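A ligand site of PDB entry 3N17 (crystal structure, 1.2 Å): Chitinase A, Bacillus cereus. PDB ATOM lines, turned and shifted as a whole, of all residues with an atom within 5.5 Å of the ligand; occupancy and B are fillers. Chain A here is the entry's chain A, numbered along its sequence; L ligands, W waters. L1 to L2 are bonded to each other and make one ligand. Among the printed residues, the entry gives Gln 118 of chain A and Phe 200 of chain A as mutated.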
ATOM      1  N   TYR A  12     -23.099  -5.767   3.063  1.00  0.00           N
ATOM      2  CA  TYR A  12     -22.000  -4.829   3.247  1.00  0.00           C
ATOM      3  C   TYR A  12     -20.963  -5.013   2.153  1.00  0.00           C
ATOM      4  O   TYR A  12     -20.643  -6.144   1.764  1.00  0.00           O
ATOM      5  CB  TYR A  12     -21.366  -4.978   4.632  1.00  0.00           C
ATOM      6  CG  TYR A  12     -22.186  -4.316   5.708  1.00  0.00           C
ATOM      7  CD1 TYR A  12     -21.883  -3.027   6.128  1.00  0.00           C
ATOM      8  CD2 TYR A  12     -23.291  -4.946   6.264  1.00  0.00           C
ATOM      9  CE1 TYR A  12     -22.653  -2.394   7.091  1.00  0.00           C
ATOM     10  CE2 TYR A  12     -24.060  -4.335   7.235  1.00  0.00           C
ATOM     11  CZ  TYR A  12     -23.726  -3.051   7.648  1.00  0.00           C
ATOM     12  OH  TYR A  12     -24.495  -2.447   8.611  1.00  0.00           O
ATOM     13  N   HIS A  14     -17.071  -4.015   0.933  1.00  0.00           N
ATOM     14  CA  HIS A  14     -15.795  -3.553   1.471  1.00  0.00           C
ATOM     15  C   HIS A  14     -15.167  -2.453   0.613  1.00  0.00           C
ATOM     16  O   HIS A  14     -14.758  -2.705  -0.521  1.00  0.00           O
ATOM     17  CB  HIS A  14     -14.749  -4.668   1.548  1.00  0.00           C
ATOM     18  CG  HIS A  14     -15.132  -5.871   2.349  1.00  0.00           C
ATOM     19  ND1 HIS A  14     -14.308  -6.961   2.449  1.00  0.00           N
ATOM     20  CD2 HIS A  14     -16.241  -6.170   3.078  1.00  0.00           C
ATOM     21  CE1 HIS A  14     -14.875  -7.884   3.208  1.00  0.00           C
ATOM     22  NE2 HIS A  14     -16.054  -7.426   3.593  1.00  0.00           N
ATOM     23  N   PHE A  16     -12.286  -1.542   0.780  1.00  0.00           N
ATOM     24  CA  PHE A  16     -10.952  -1.880   1.252  1.00  0.00           C
ATOM     25  C   PHE A  16     -10.706  -3.339   0.903  1.00  0.00           C
ATOM     26  O   PHE A  16     -11.663  -4.094   0.676  1.00  0.00           O
ATOM     27  CB  PHE A  16     -10.853  -1.690   2.766  1.00  0.00           C
ATOM     28  CG  PHE A  16     -11.889  -2.458   3.545  1.00  0.00           C
ATOM     29  CD1 PHE A  16     -11.690  -3.789   3.892  1.00  0.00           C
ATOM     30  CD2 PHE A  16     -13.065  -1.843   3.939  1.00  0.00           C
ATOM     31  CE1 PHE A  16     -12.659  -4.485   4.612  1.00  0.00           C
ATOM     32  CE2 PHE A  16     -14.025  -2.532   4.652  1.00  0.00           C
ATOM     33  CZ  PHE A  16     -13.827  -3.856   4.992  1.00  0.00           C
ATOM     34  N   ASN A  18      -9.357  -6.633   2.515  1.00  0.00           N
ATOM     35  CA  ASN A  18      -8.919  -7.323   3.723  1.00  0.00           C
ATOM     36  C   ASN A  18      -8.473  -8.748   3.434  1.00  0.00           C
ATOM     37  O   ASN A  18      -8.403  -9.572   4.346  1.00  0.00           O
ATOM     38  CB  ASN A  18     -10.028  -7.320   4.788  1.00  0.00           C
ATOM     39  CG  ASN A  18     -11.190  -8.217   4.427  1.00  0.00           C
ATOM     40  OD1 ASN A  18     -11.301  -8.692   3.291  1.00  0.00           O
ATOM     41  ND2 ASN A  18     -12.079  -8.454   5.392  1.00  0.00           N
ATOM     42  N   PHE A  39     -16.266   1.826   4.767  1.00  0.00           N
ATOM     43  CA  PHE A  39     -17.086   2.652   5.667  1.00  0.00           C
ATOM     44  C   PHE A  39     -16.678   4.120   5.535  1.00  0.00           C
ATOM     45  O   PHE A  39     -15.536   4.439   5.166  1.00  0.00           O
ATOM     46  CB  PHE A  39     -16.821   2.282   7.128  1.00  0.00           C
ATOM     47  CG  PHE A  39     -17.220   0.886   7.490  1.00  0.00           C
ATOM     48  CD1 PHE A  39     -16.289  -0.121   7.579  1.00  0.00           C
ATOM     49  CD2 PHE A  39     -18.544   0.598   7.789  1.00  0.00           C
ATOM     50  CE1 PHE A  39     -16.664  -1.403   7.923  1.00  0.00           C
ATOM     51  CE2 PHE A  39     -18.929  -0.677   8.141  1.00  0.00           C
ATOM     52  CZ  PHE A  39     -17.989  -1.677   8.208  1.00  0.00           C
ATOM     53  N   GLU A  41     -15.386   6.941   7.740  1.00  0.00           N
ATOM     54  CA  GLU A  41     -14.663   7.004   9.018  1.00  0.00           C
ATOM     55  C   GLU A  41     -14.219   8.444   9.269  1.00  0.00           C
ATOM     56  O   GLU A  41     -14.531   9.338   8.492  1.00  0.00           O
ATOM     57  CB  GLU A  41     -13.475   6.028   9.011  1.00  0.00           C
ATOM     58  CG  GLU A  41     -13.878   4.570   8.782  1.00  0.00           C
ATOM     59  CD  GLU A  41     -12.700   3.614   8.781  1.00  0.00           C
ATOM     60  OE1 GLU A  41     -11.620   3.974   9.289  1.00  0.00           O
ATOM     61  OE2 GLU A  41     -12.862   2.477   8.277  1.00  0.00           O
ATOM     62  N   SER A  78     -22.306   3.356   4.854  1.00  0.00           N
ATOM     63  CA  SER A  78     -22.218   2.903   6.234  1.00  0.00           C
ATOM     64  C   SER A  78     -21.155   3.682   6.997  1.00  0.00           C
ATOM     65  O   SER A  78     -20.028   3.863   6.526  1.00  0.00           O
ATOM     66  CB  SER A  78     -21.924   1.404   6.310  1.00  0.00           C
ATOM     67  OG  SER A  78     -21.937   0.968   7.670  1.00  0.00           O
ATOM     68  N   GLY A  80     -18.889   4.040  10.379  1.00  0.00           N
ATOM     69  CA  GLY A  80     -18.324   3.391  11.549  1.00  0.00           C
ATOM     70  C   GLY A  80     -17.547   2.142  11.201  1.00  0.00           C
ATOM     71  O   GLY A  80     -16.424   2.208  10.706  1.00  0.00           O
ATOM     72  N   GLY A  81     -18.159   0.987  11.445  1.00  0.00           N
ATOM     73  CA  GLY A  81     -17.469  -0.281  11.275  1.00  0.00           C
ATOM     74  C   GLY A  81     -16.531  -0.565  12.436  1.00  0.00           C
ATOM     75  O   GLY A  81     -16.523   0.141  13.438  1.00  0.00           O
ATOM     76  N   GLN A  82     -15.741  -1.623  12.294  1.00  0.00           N
ATOM     77  CA  GLN A  82     -14.848  -2.018  13.367  1.00  0.00           C
ATOM     78  C   GLN A  82     -13.916  -0.881  13.800  1.00  0.00           C
ATOM     79  O   GLN A  82     -13.640  -0.722  14.987  1.00  0.00           O
ATOM     80  CB  GLN A  82     -14.033  -3.239  12.947  1.00  0.00           C
ATOM     81  CG  GLN A  82     -13.199  -3.863  14.057  1.00  0.00           C
ATOM     82  CD  GLN A  82     -12.628  -5.208  13.658  1.00  0.00           C
ATOM     83  OE1 GLN A  82     -13.366  -6.159  13.400  1.00  0.00           O
ATOM     84  NE2 GLN A  82     -11.303  -5.301  13.605  1.00  0.00           N
ATOM     85  N   ASN A  83     -13.434  -0.104  12.842  1.00  0.00           N
ATOM     86  CA  ASN A  83     -12.377   0.877  13.109  1.00  0.00           C
ATOM     87  C   ASN A  83     -12.847   2.330  13.178  1.00  0.00           C
ATOM     88  O   ASN A  83     -12.093   3.210  13.600  1.00  0.00           O
ATOM     89  CB  ASN A  83     -11.252   0.749  12.076  1.00  0.00           C
ATOM     90  CG  ASN A  83     -10.665  -0.641  12.032  1.00  0.00           C
ATOM     91  OD1 ASN A  83     -10.411  -1.189  10.959  1.00  0.00           O
ATOM     92  ND2 ASN A  83     -10.452  -1.236  13.204  1.00  0.00           N
ATOM     93  N   ASP A 116     -23.381   2.258  11.928  1.00  0.00           N
ATOM     94  CA  ASP A 116     -22.649   1.066  12.280  1.00  0.00           C
ATOM     95  C   ASP A 116     -21.553   1.422  13.290  1.00  0.00           C
ATOM     96  O   ASP A 116     -20.404   1.026  13.129  1.00  0.00           O
ATOM     97  CB  ASP A 116     -22.027   0.522  10.997  1.00  0.00           C
ATOM     98  CG  ASP A 116     -21.695  -0.940  11.065  1.00  0.00           C
ATOM     99  OD1 ASP A 116     -21.604  -1.515  12.166  1.00  0.00           O
ATOM    100  OD2 ASP A 116     -21.500  -1.519   9.979  1.00  0.00           O
ATOM    101  N   GLN A 118     -19.541   1.214  16.637  1.00  0.00           N
ATOM    102  CA  GLN A 118     -19.266   0.104  17.557  1.00  0.00           C
ATOM    103  C   GLN A 118     -18.350   0.498  18.708  1.00  0.00           C
ATOM    104  O   GLN A 118     -17.830  -0.352  19.418  1.00  0.00           O
ATOM    105  CB  GLN A 118     -18.687  -1.084  16.784  1.00  0.00           C
ATOM    106  CG  GLN A 118     -19.607  -1.590  15.693  1.00  0.00           C
ATOM    107  CD  GLN A 118     -18.973  -2.686  14.853  1.00  0.00           C
ATOM    108  OE1 GLN A 118     -17.969  -3.283  15.239  1.00  0.00           O
ATOM    109  NE2 GLN A 118     -19.574  -2.959  13.701  1.00  0.00           N
ATOM    110  N   ALA A 161     -26.779  -1.085  12.409  1.00  0.00           N
ATOM    111  CA  ALA A 161     -26.260  -2.425  12.676  1.00  0.00           C
ATOM    112  C   ALA A 161     -25.550  -2.509  14.023  1.00  0.00           C
ATOM    113  O   ALA A 161     -24.361  -2.845  14.093  1.00  0.00           O
ATOM    114  CB  ALA A 161     -25.322  -2.856  11.563  1.00  0.00           C
ATOM    115  N   GLN A 198     -26.279  -7.195  14.536  1.00  0.00           N
ATOM    116  CA  GLN A 198     -25.273  -8.199  14.199  1.00  0.00           C
ATOM    117  C   GLN A 198     -25.414  -9.414  15.112  1.00  0.00           C
ATOM    118  O   GLN A 198     -24.962  -9.389  16.260  1.00  0.00           O
ATOM    119  CB  GLN A 198     -23.879  -7.610  14.313  1.00  0.00           C
ATOM    120  CG  GLN A 198     -23.668  -6.382  13.449  1.00  0.00           C
ATOM    121  CD  GLN A 198     -22.239  -5.901  13.460  1.00  0.00           C
ATOM    122  OE1 GLN A 198     -21.310  -6.694  13.407  1.00  0.00           O
ATOM    123  NE2 GLN A 198     -22.061  -4.587  13.527  1.00  0.00           N
ATOM    124  N   PHE A 200     -23.767 -11.929  15.478  1.00  0.00           N
ATOM    125  CA  PHE A 200     -22.503 -12.644  15.341  1.00  0.00           C
ATOM    126  C   PHE A 200     -21.387 -11.920  16.090  1.00  0.00           C
ATOM    127  O   PHE A 200     -21.558 -10.768  16.491  1.00  0.00           O
ATOM    128  CB  PHE A 200     -22.148 -12.882  13.866  1.00  0.00           C
ATOM    129  CG  PHE A 200     -22.148 -11.635  13.017  1.00  0.00           C
ATOM    130  CD1 PHE A 200     -20.994 -10.890  12.867  1.00  0.00           C
ATOM    131  CD2 PHE A 200     -23.287 -11.238  12.343  1.00  0.00           C
ATOM    132  CE1 PHE A 200     -20.978  -9.761  12.072  1.00  0.00           C
ATOM    133  CE2 PHE A 200     -23.281 -10.103  11.540  1.00  0.00           C
ATOM    134  CZ  PHE A 200     -22.126  -9.364  11.412  1.00  0.00           C
ATOM    135  N   ASN A 201     -20.251 -12.603  16.250  1.00  0.00           N
ATOM    136  CA  ASN A 201     -19.218 -12.203  17.196  1.00  0.00           C
ATOM    137  C   ASN A 201     -19.873 -11.794  18.519  1.00  0.00           C
ATOM    138  O   ASN A 201     -19.484 -10.791  19.131  1.00  0.00           O
ATOM    139  CB  ASN A 201     -18.359 -11.054  16.631  1.00  0.00           C
ATOM    140  CG  ASN A 201     -17.717 -11.400  15.299  1.00  0.00           C
ATOM    141  OD1 ASN A 201     -17.137 -12.476  15.125  1.00  0.00           O
ATOM    142  ND2 ASN A 201     -17.793 -10.472  14.349  1.00  0.00           N
ATOM    143  N   ALA A 259     -15.697 -17.668   8.168  1.00  0.00           N
ATOM    144  CA  ALA A 259     -14.576 -16.762   8.402  1.00  0.00           C
ATOM    145  C   ALA A 259     -14.968 -15.286   8.434  1.00  0.00           C
ATOM    146  O   ALA A 259     -14.163 -14.434   8.814  1.00  0.00           O
ATOM    147  CB  ALA A 259     -13.486 -16.992   7.359  1.00  0.00           C
ATOM    148  N   ALA A 260     -16.189 -14.970   8.018  1.00  0.00           N
ATOM    149  CA  ALA A 260     -16.647 -13.582   8.011  1.00  0.00           C
ATOM    150  C   ALA A 260     -16.866 -13.050   9.424  1.00  0.00           C
ATOM    151  O   ALA A 260     -16.882 -11.833   9.631  1.00  0.00           O
ATOM    152  CB  ALA A 260     -17.915 -13.438   7.177  1.00  0.00           C
ATOM    153  N   ALA A 261     -17.031 -13.954  10.384  1.00  0.00           N
ATOM    154  CA  ALA A 261     -17.171 -13.609  11.796  1.00  0.00           C
ATOM    155  C   ALA A 261     -16.247 -14.507  12.616  1.00  0.00           C
ATOM    156  O   ALA A 261     -16.662 -15.567  13.074  1.00  0.00           O
ATOM    157  CB  ALA A 261     -18.621 -13.756  12.247  1.00  0.00           C
ATOM    158  N   PRO A 262     -14.994 -14.079  12.794  1.00  0.00           N
ATOM    159  CA  PRO A 262     -13.965 -14.944  13.379  1.00  0.00           C
ATOM    160  C   PRO A 262     -14.226 -15.405  14.813  1.00  0.00           C
ATOM    161  O   PRO A 262     -13.565 -16.342  15.269  1.00  0.00           O
ATOM    162  CB  PRO A 262     -12.705 -14.084  13.330  1.00  0.00           C
ATOM    163  CG  PRO A 262     -12.956 -13.090  12.273  1.00  0.00           C
ATOM    164  CD  PRO A 262     -14.430 -12.814  12.300  1.00  0.00           C
ATOM    165  N   MET A 304     -29.499  -9.233   6.557  1.00  0.00           N
ATOM    166  CA  MET A 304     -28.297  -8.484   6.244  1.00  0.00           C
ATOM    167  C   MET A 304     -27.098  -9.435   6.370  1.00  0.00           C
ATOM    168  O   MET A 304     -27.143 -10.403   7.125  1.00  0.00           O
ATOM    169  CB  MET A 304     -28.151  -7.318   7.229  1.00  0.00           C
ATOM    170  CG  MET A 304     -26.815  -6.595   7.198  1.00  0.00           C
ATOM    171  SD  MET A 304     -25.492  -7.420   8.146  1.00  0.00           S
ATOM    172  CE  MET A 304     -25.623  -6.615   9.741  1.00  0.00           C
ATOM    173  N   TRP A 306     -22.639  -9.449   6.665  1.00  0.00           N
ATOM    174  CA  TRP A 306     -21.243  -9.160   6.485  1.00  0.00           C
ATOM    175  C   TRP A 306     -20.670 -10.409   5.807  1.00  0.00           C
ATOM    176  O   TRP A 306     -20.493 -11.434   6.470  1.00  0.00           O
ATOM    177  CB  TRP A 306     -20.557  -8.940   7.829  1.00  0.00           C
ATOM    178  CG  TRP A 306     -19.149  -8.489   7.637  1.00  0.00           C
ATOM    179  CD1 TRP A 306     -18.020  -9.261   7.701  1.00  0.00           C
ATOM    180  CD2 TRP A 306     -18.726  -7.177   7.291  1.00  0.00           C
ATOM    181  NE1 TRP A 306     -16.919  -8.494   7.409  1.00  0.00           N
ATOM    182  CE2 TRP A 306     -17.324  -7.212   7.165  1.00  0.00           C
ATOM    183  CE3 TRP A 306     -19.397  -5.970   7.073  1.00  0.00           C
ATOM    184  CZ2 TRP A 306     -16.581  -6.082   6.822  1.00  0.00           C
ATOM    185  CZ3 TRP A 306     -18.654  -4.847   6.737  1.00  0.00           C
ATOM    186  CH2 TRP A 306     -17.261  -4.911   6.626  1.00  0.00           C
ATOM    187  N   TRP A 310     -17.260 -11.405   1.356  1.00  0.00           N
ATOM    188  CA  TRP A 310     -17.139 -12.740   1.924  1.00  0.00           C
ATOM    189  C   TRP A 310     -18.031 -13.743   1.203  1.00  0.00           C
ATOM    190  O   TRP A 310     -17.638 -14.886   0.976  1.00  0.00           O
ATOM    191  CB  TRP A 310     -17.443 -12.719   3.426  1.00  0.00           C
ATOM    192  CG  TRP A 310     -16.259 -12.364   4.265  1.00  0.00           C
ATOM    193  CD1 TRP A 310     -16.075 -11.219   4.982  1.00  0.00           C
ATOM    194  CD2 TRP A 310     -15.077 -13.151   4.450  1.00  0.00           C
ATOM    195  NE1 TRP A 310     -14.854 -11.259   5.614  1.00  0.00           N
ATOM    196  CE2 TRP A 310     -14.221 -12.429   5.308  1.00  0.00           C
ATOM    197  CE3 TRP A 310     -14.662 -14.407   3.979  1.00  0.00           C
ATOM    198  CZ2 TRP A 310     -12.971 -12.914   5.701  1.00  0.00           C
ATOM    199  CZ3 TRP A 310     -13.423 -14.879   4.371  1.00  0.00           C
ATOM    200  CH2 TRP A 310     -12.598 -14.138   5.222  1.00  0.00           C
HETATM  201  C1  LIG L   1     -18.016  -6.024  12.764  1.00  0.00           C
HETATM  202  C2  LIG L   1     -18.287  -5.056  11.601  1.00  0.00           C
HETATM  203  C3  LIG L   1     -17.193  -5.152  10.546  1.00  0.00           C
HETATM  204  C4  LIG L   1     -16.301  -6.344  10.861  1.00  0.00           C
HETATM  205  C5  LIG L   1     -17.170  -7.566  11.166  1.00  0.00           C
HETATM  206  C6  LIG L   1     -16.316  -8.830  11.320  1.00  0.00           C
HETATM  207  C7  LIG L   1     -20.392  -4.692  10.309  1.00  0.00           C
HETATM  208  C8  LIG L   1     -21.782  -5.206  10.071  1.00  0.00           C
HETATM  209  N1  LIG L   1     -19.597  -5.413  11.096  1.00  0.00           N
HETATM  210  O1  LIG L   1     -16.833  -5.688  13.462  1.00  0.00           O
HETATM  211  O2  LIG L   1     -16.441  -3.948  10.505  1.00  0.00           O
HETATM  212  O3  LIG L   1     -15.507  -6.683   9.746  1.00  0.00           O
HETATM  213  O4  LIG L   1     -17.956  -7.367  12.328  1.00  0.00           O
HETATM  214  O5  LIG L   1     -17.140  -9.944  11.614  1.00  0.00           O
HETATM  215  O6  LIG L   1     -20.038  -3.651   9.767  1.00  0.00           O
HETATM  216  C1  LG2 L   2     -14.191  -6.143   9.793  1.00  0.00           C
HETATM  217  C2  LG2 L   2     -13.298  -7.014   8.915  1.00  0.00           C
HETATM  218  C3  LG2 L   2     -11.896  -6.425   8.824  1.00  0.00           C
HETATM  219  C4  LG2 L   2     -11.981  -4.963   8.400  1.00  0.00           C
HETATM  220  C5  LG2 L   2     -12.928  -4.206   9.325  1.00  0.00           C
HETATM  221  C6  LG2 L   2     -13.083  -2.754   8.909  1.00  0.00           C
HETATM  222  C7  LG2 L   2     -13.606  -9.419   8.631  1.00  0.00           C
HETATM  223  C8  LG2 L   2     -13.403 -10.777   9.241  1.00  0.00           C
HETATM  224  N1  LG2 L   2     -13.257  -8.378   9.392  1.00  0.00           N
HETATM  225  O1  LG2 L   2     -11.151  -7.151   7.871  1.00  0.00           O
HETATM  226  O2  LG2 L   2     -10.698  -4.361   8.437  1.00  0.00           O
HETATM  227  O3  LG2 L   2     -14.190  -4.828   9.295  1.00  0.00           O
HETATM  228  O4  LG2 L   2     -13.964  -2.115   9.816  1.00  0.00           O
HETATM  229  O5  LG2 L   2     -14.075  -9.302   7.507  1.00  0.00           O
HETATM  230  O   HOH W   1     -12.508  -8.498  12.127  1.00  0.00           O
HETATM  231  O   HOH W   2     -19.883  -7.751  10.421  1.00  0.00           O
HETATM  232  O   HOH W   3      -9.207  -3.814  10.576  1.00  0.00           O
HETATM  233  O   HOH W   4     -14.205   0.657  10.036  1.00  0.00           O
HETATM  234  O   HOH W   5      -8.987  -4.622   6.426  1.00  0.00           O
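Water W2 lies within hydrogen-bond range of N1 of LIG L1 and OE1 of Gln 198.
Water W3 lies within hydrogen-bond range of O2 of LG2 L2 (2.7 Å) and OD1 of Asn 83 (2.9 Å).
Water W4 lies within hydrogen-bond range of O of Gly 80 (2.8 Å), O4 of LG2 L2 (2.8 Å), OE2 of Glu 41 (2.9 Å) and N of Asn 83 (3.0 Å).
Water W1 lies within hydrogen-bond range of OE1 of Gln 82 (2.8 Å) and N1 of LG2 L2 (2.8 Å).
CE2 of Tyr 12 touches C8 of LIG L1 (3.7 Å).
CE1 of Phe 16 touches C4 of LG2 L2, 3.9 Å away.
CZ of Phe 39 touches O6 of LIG L1, 3.2 Å away.
CA of Gly 81 touches O2 of LIG L1 (3.9 Å).
Asn 83 touches the ligand.
CE1 of Phe 200 touches O4 of LIG L1, 3.9 Å away.
O of Ala 259 touches C8 of LG2 L2, at 3.8 Å.
CA of Ala 261 touches O5 of LIG L1, at 3.7 Å.
CD of Pro 262 touches C8 of LG2 L2, at 3.8 Å.
18 residues have an atom within 4 Å of the ligand: Tyr 12, Phe 16, Asn 18, Phe 39, Gly 81, Gln 82, Asn 83, Asp 116, Gln 118, Gln 198, Phe 200, Asn 201, Ala 259, Ala 260, Ala 261, Pro 262, Trp 306 and Trp 310.
The nearest printed residue that does not touch the ligand is Met 304 (4.1 Å).
The side-chain carboxylate (OD1) of Asp 116 lies within hydrogen-bond range of the side-chain amide nitrogen (NE2) of Gln 198, 3.4 Å away.
The side-chain amide nitrogen (NE2) of Gln 118 sits at hydrogen-bond distance from the side-chain carboxylate (OD1) of Asp 116.
The side-chain carboxylate of Asp 116 sits close to the side-chain hydroxyl of Tyr 12, 3.4 Å away.
The backbone carbonyl oxygen (O) of Asp 116 is in hydrogen-bond range of the backbone NH (N) of Gly 81, 2.8 Å away.
OD2 of Asp 116 lies close to OG of Ser 78, 3.4 Å away.
NE2 of Gln 198 lies close to NE2 of Gln 118 (3.0 Å).
The backbone carbonyl oxygen (O) of Ala 161 lies within hydrogen-bond range of the side-chain amide nitrogen (NE2) of Gln 198, at 2.9 Å.
An oxygen (O6) of LIG L1 lies close to the side-chain carboxylate (OD2) of Asp 116.
An oxygen (O5) of LIG L1 sits at hydrogen-bond distance from the backbone carbonyl oxygen (O) of Ala 260 (2.8 Å).
An oxygen (O5) of LG2 L2 is in hydrogen-bond range of the indole nitrogen of Trp 310, 2.8 Å away.
The side-chain amide nitrogen (ND2) of Asn 201 sits at hydrogen-bond distance from an oxygen (O5) of LIG L1 (2.9 Å).
The side-chain amide nitrogen (ND2) of Asn 18 lies within hydrogen-bond range of an oxygen (O1) of LG2 L2 (3.0 Å).
NE1 of Trp 306 is in hydrogen-bond range of O5 of LG2 L2.
N of Gln 82 sits at hydrogen-bond distance from O2 of LIG L1, 3.0 Å away.
The side-chain amide oxygen (OE1) of Gln 82 lies within hydrogen-bond range of an oxygen (O1) of LIG L1 (3.5 Å).
OE1 of Gln 198 is in hydrogen-bond range of N1 of LIG L1, at 3.1 Å.
The side-chain amide oxygen (OE1) of Gln 118 sits at hydrogen-bond distance from an oxygen (O1) of LIG L1, 3.2 Å away.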
